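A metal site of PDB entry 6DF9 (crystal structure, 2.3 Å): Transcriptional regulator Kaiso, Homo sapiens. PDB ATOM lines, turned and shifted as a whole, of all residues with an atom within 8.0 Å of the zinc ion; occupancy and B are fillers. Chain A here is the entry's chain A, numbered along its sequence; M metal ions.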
ATOM      1  N   GLN A  81     -34.771 -22.063  17.702  1.00  0.00           N
ATOM      2  CA  GLN A  81     -34.109 -22.897  18.698  1.00  0.00           C
ATOM      3  C   GLN A  81     -32.606 -22.999  18.485  1.00  0.00           C
ATOM      4  O   GLN A  81     -32.134 -23.303  17.393  1.00  0.00           O
ATOM      5  CB  GLN A  81     -34.765 -24.289  18.744  1.00  0.00           C
ATOM      6  CG  GLN A  81     -34.077 -25.220  19.762  1.00  0.00           C
ATOM      7  CD  GLN A  81     -34.741 -26.579  19.862  1.00  0.00           C
ATOM      8  OE1 GLN A  81     -35.213 -27.135  18.865  1.00  0.00           O
ATOM      9  NE2 GLN A  81     -34.790 -27.115  21.074  1.00  0.00           N
ATOM     10  N   CYS A  82     -31.853 -22.721  19.554  1.00  0.00           N
ATOM     11  CA  CYS A  82     -30.403 -22.871  19.539  1.00  0.00           C
ATOM     12  C   CYS A  82     -30.029 -24.352  19.463  1.00  0.00           C
ATOM     13  O   CYS A  82     -30.474 -25.184  20.289  1.00  0.00           O
ATOM     14  CB  CYS A  82     -29.781 -22.216  20.775  1.00  0.00           C
ATOM     15  SG  CYS A  82     -28.031 -22.658  21.064  1.00  0.00           S
ATOM     16  N   LEU A  83     -29.207 -24.694  18.477  1.00  0.00           N
ATOM     17  CA  LEU A  83     -28.888 -26.101  18.273  1.00  0.00           C
ATOM     18  C   LEU A  83     -27.747 -26.534  19.177  1.00  0.00           C
ATOM     19  O   LEU A  83     -27.491 -27.723  19.337  1.00  0.00           O
ATOM     20  CB  LEU A  83     -28.559 -26.392  16.809  1.00  0.00           C
ATOM     21  CG  LEU A  83     -29.748 -26.270  15.844  1.00  0.00           C
ATOM     22  CD1 LEU A  83     -29.391 -26.706  14.440  1.00  0.00           C
ATOM     23  CD2 LEU A  83     -30.927 -27.061  16.337  1.00  0.00           C
ATOM     24  N   ALA A  84     -27.086 -25.574  19.820  1.00  0.00           N
ATOM     25  CA  ALA A  84     -25.961 -25.895  20.688  1.00  0.00           C
ATOM     26  C   ALA A  84     -26.417 -26.342  22.096  1.00  0.00           C
ATOM     27  O   ALA A  84     -25.705 -27.100  22.739  1.00  0.00           O
ATOM     28  CB  ALA A  84     -25.002 -24.691  20.791  1.00  0.00           C
ATOM     29  N   CYS A  85     -27.580 -25.876  22.558  1.00  0.00           N
ATOM     30  CA  CYS A  85     -28.007 -26.158  23.928  1.00  0.00           C
ATOM     31  C   CYS A  85     -29.525 -26.366  24.032  1.00  0.00           C
ATOM     32  O   CYS A  85     -30.045 -26.661  25.091  1.00  0.00           O
ATOM     33  CB  CYS A  85     -27.594 -25.035  24.879  1.00  0.00           C
ATOM     34  SG  CYS A  85     -28.665 -23.596  24.708  1.00  0.00           S
ATOM     35  N   GLY A  86     -30.241 -26.166  22.928  1.00  0.00           N
ATOM     36  CA  GLY A  86     -31.655 -26.430  22.894  1.00  0.00           C
ATOM     37  C   GLY A  86     -32.629 -25.330  23.299  1.00  0.00           C
ATOM     38  O   GLY A  86     -33.823 -25.519  23.137  1.00  0.00           O
ATOM     39  N   LYS A  87     -32.143 -24.214  23.842  1.00  0.00           N
ATOM     40  CA  LYS A  87     -33.017 -23.116  24.238  1.00  0.00           C
ATOM     41  C   LYS A  87     -33.765 -22.557  23.054  1.00  0.00           C
ATOM     42  O   LYS A  87     -33.254 -22.499  21.943  1.00  0.00           O
ATOM     43  CB  LYS A  87     -32.250 -21.993  24.931  1.00  0.00           C
ATOM     44  CG  LYS A  87     -31.918 -22.277  26.397  1.00  0.00           C
ATOM     45  CD  LYS A  87     -31.188 -21.103  27.029  1.00  0.00           C
ATOM     46  CE  LYS A  87     -30.548 -21.472  28.372  1.00  0.00           C
ATOM     47  NZ  LYS A  87     -31.503 -21.452  29.525  1.00  0.00           N
ATOM     48  N   SER A  88     -34.998 -22.137  23.308  1.00  0.00           N
ATOM     49  CA  SER A  88     -35.837 -21.587  22.260  1.00  0.00           C
ATOM     50  C   SER A  88     -36.134 -20.114  22.496  1.00  0.00           C
ATOM     51  O   SER A  88     -36.125 -19.651  23.643  1.00  0.00           O
ATOM     52  CB  SER A  88     -37.110 -22.401  22.146  1.00  0.00           C
ATOM     53  OG  SER A  88     -36.791 -23.694  21.703  1.00  0.00           O
ATOM     54  N   PHE A  89     -36.403 -19.392  21.418  1.00  0.00           N
ATOM     55  CA  PHE A  89     -36.563 -17.929  21.444  1.00  0.00           C
ATOM     56  C   PHE A  89     -37.687 -17.526  20.534  1.00  0.00           C
ATOM     57  O   PHE A  89     -38.005 -18.251  19.574  1.00  0.00           O
ATOM     58  CB  PHE A  89     -35.246 -17.239  21.041  1.00  0.00           C
ATOM     59  CG  PHE A  89     -34.104 -17.667  21.888  1.00  0.00           C
ATOM     60  CD1 PHE A  89     -33.824 -17.009  23.085  1.00  0.00           C
ATOM     61  CD2 PHE A  89     -33.346 -18.793  21.543  1.00  0.00           C
ATOM     62  CE1 PHE A  89     -32.796 -17.438  23.921  1.00  0.00           C
ATOM     63  CE2 PHE A  89     -32.302 -19.237  22.361  1.00  0.00           C
ATOM     64  CZ  PHE A  89     -32.031 -18.556  23.555  1.00  0.00           C
ATOM     65  N   MET A  95     -32.444 -15.082  19.720  1.00  0.00           N
ATOM     66  CA  MET A  95     -31.678 -16.275  19.403  1.00  0.00           C
ATOM     67  C   MET A  95     -30.235 -15.882  19.057  1.00  0.00           C
ATOM     68  O   MET A  95     -29.280 -16.456  19.595  1.00  0.00           O
ATOM     69  CB  MET A  95     -32.348 -17.031  18.236  1.00  0.00           C
ATOM     70  CG  MET A  95     -31.527 -18.228  17.644  1.00  0.00           C
ATOM     71  SD  MET A  95     -30.175 -17.614  16.515  1.00  0.00           S
ATOM     72  CE  MET A  95     -31.062 -17.066  15.057  1.00  0.00           C
ATOM     73  N   HIS A  98     -28.253 -14.628  21.954  1.00  0.00           N
ATOM     74  CA  HIS A  98     -27.960 -15.749  22.842  1.00  0.00           C
ATOM     75  C   HIS A  98     -26.740 -16.494  22.320  1.00  0.00           C
ATOM     76  O   HIS A  98     -25.764 -16.701  23.036  1.00  0.00           O
ATOM     77  CB  HIS A  98     -29.167 -16.719  22.961  1.00  0.00           C
ATOM     78  CG  HIS A  98     -28.772 -18.110  23.388  1.00  0.00           C
ATOM     79  ND1 HIS A  98     -28.602 -18.465  24.713  1.00  0.00           N
ATOM     80  CD2 HIS A  98     -28.545 -19.242  22.673  1.00  0.00           C
ATOM     81  CE1 HIS A  98     -28.265 -19.741  24.793  1.00  0.00           C
ATOM     82  NE2 HIS A  98     -28.220 -20.231  23.562  1.00  0.00           N
ATOM     83  N   ILE A  99     -26.795 -16.899  21.056  1.00  0.00           N
ATOM     84  CA  ILE A  99     -25.708 -17.668  20.480  1.00  0.00           C
ATOM     85  C   ILE A  99     -24.386 -16.908  20.493  1.00  0.00           C
ATOM     86  O   ILE A  99     -23.340 -17.485  20.786  1.00  0.00           O
ATOM     87  CB  ILE A  99     -26.049 -18.100  19.043  1.00  0.00           C
ATOM     88  CG1 ILE A  99     -27.256 -19.041  19.086  1.00  0.00           C
ATOM     89  CG2 ILE A  99     -24.855 -18.773  18.388  1.00  0.00           C
ATOM     90  CD1 ILE A  99     -27.537 -19.740  17.777  1.00  0.00           C
ATOM     91  N   LYS A 100     -24.438 -15.609  20.219  1.00  0.00           N
ATOM     92  CA  LYS A 100     -23.221 -14.811  20.253  1.00  0.00           C
ATOM     93  C   LYS A 100     -22.642 -14.729  21.660  1.00  0.00           C
ATOM     94  O   LYS A 100     -21.431 -14.865  21.850  1.00  0.00           O
ATOM     95  CB  LYS A 100     -23.481 -13.402  19.714  1.00  0.00           C
ATOM     96  CG  LYS A 100     -23.608 -13.356  18.199  1.00  0.00           C
ATOM     97  CD  LYS A 100     -23.844 -11.920  17.723  1.00  0.00           C
ATOM     98  CE  LYS A 100     -23.988 -11.823  16.208  1.00  0.00           C
ATOM     99  NZ  LYS A 100     -24.351 -10.452  15.739  1.00  0.00           N
ATOM    100  N   VAL A 102     -23.488 -16.551  24.570  1.00  0.00           N
ATOM    101  CA  VAL A 102     -23.308 -17.785  25.327  1.00  0.00           C
ATOM    102  C   VAL A 102     -22.344 -18.735  24.601  1.00  0.00           C
ATOM    103  O   VAL A 102     -21.558 -19.451  25.244  1.00  0.00           O
ATOM    104  CB  VAL A 102     -24.670 -18.495  25.599  1.00  0.00           C
ATOM    105  CG1 VAL A 102     -24.456 -19.878  26.155  1.00  0.00           C
ATOM    106  CG2 VAL A 102     -25.524 -17.669  26.561  1.00  0.00           C
ATOM    107  N   HIS A 103     -22.395 -18.742  23.270  1.00  0.00           N
ATOM    108  CA  HIS A 103     -21.654 -19.738  22.516  1.00  0.00           C
ATOM    109  C   HIS A 103     -20.498 -19.166  21.695  1.00  0.00           C
ATOM    110  O   HIS A 103     -19.792 -19.916  21.023  1.00  0.00           O
ATOM    111  CB  HIS A 103     -22.606 -20.509  21.616  1.00  0.00           C
ATOM    112  CG  HIS A 103     -23.674 -21.235  22.371  1.00  0.00           C
ATOM    113  ND1 HIS A 103     -23.382 -22.217  23.303  1.00  0.00           N
ATOM    114  CD2 HIS A 103     -25.021 -21.122  22.352  1.00  0.00           C
ATOM    115  CE1 HIS A 103     -24.517 -22.673  23.824  1.00  0.00           C
ATOM    116  NE2 HIS A 103     -25.519 -22.027  23.265  1.00  0.00           N
ATOM    117  N   LEU A 113     -26.675 -22.760  13.174  1.00  0.00           N
ATOM    118  CA  LEU A 113     -26.496 -22.853  14.597  1.00  0.00           C
ATOM    119  C   LEU A 113     -27.862 -22.847  15.253  1.00  0.00           C
ATOM    120  O   LEU A 113     -27.993 -22.954  16.472  1.00  0.00           O
ATOM    121  CB  LEU A 113     -25.635 -21.695  15.106  1.00  0.00           C
ATOM    122  CG  LEU A 113     -24.251 -21.581  14.439  1.00  0.00           C
ATOM    123  CD1 LEU A 113     -23.370 -20.522  15.064  1.00  0.00           C
ATOM    124  CD2 LEU A 113     -23.541 -22.921  14.468  1.00  0.00           C
HETATM  125 ZN    ZN M   1     -27.588 -22.164  23.204  1.00  0.00          ZN
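The zinc ion is bound by a ring nitrogen (NE2) of His 98 (2.1 Å).
NE2 of His 103 binds the zinc ion.
The zinc ion is bound by SG of Cys 82.
The zinc ion is bound by the side-chain sulfur (SG) of Cys 85 (2.3 Å).
The zinc ion has four donor atoms within binding distance.
The side-chain sulfur (SG) of Cys 82 sits close to the backbone NH (N) of Ala 84.
The backbone carbonyl oxygen of Lys 87 sits at hydrogen-bond distance from the backbone NH of Cys 82.
The side-chain sulfur (SG) of Cys 85 sits close to the backbone NH (N) of Lys 87 (3.6 Å).
Within 4 Å of the zinc ion: Cys 82, Cys 85, His 98 and His 103.
Along chain A the residues within 4 Å of the zinc ion span positions 82 to 103.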
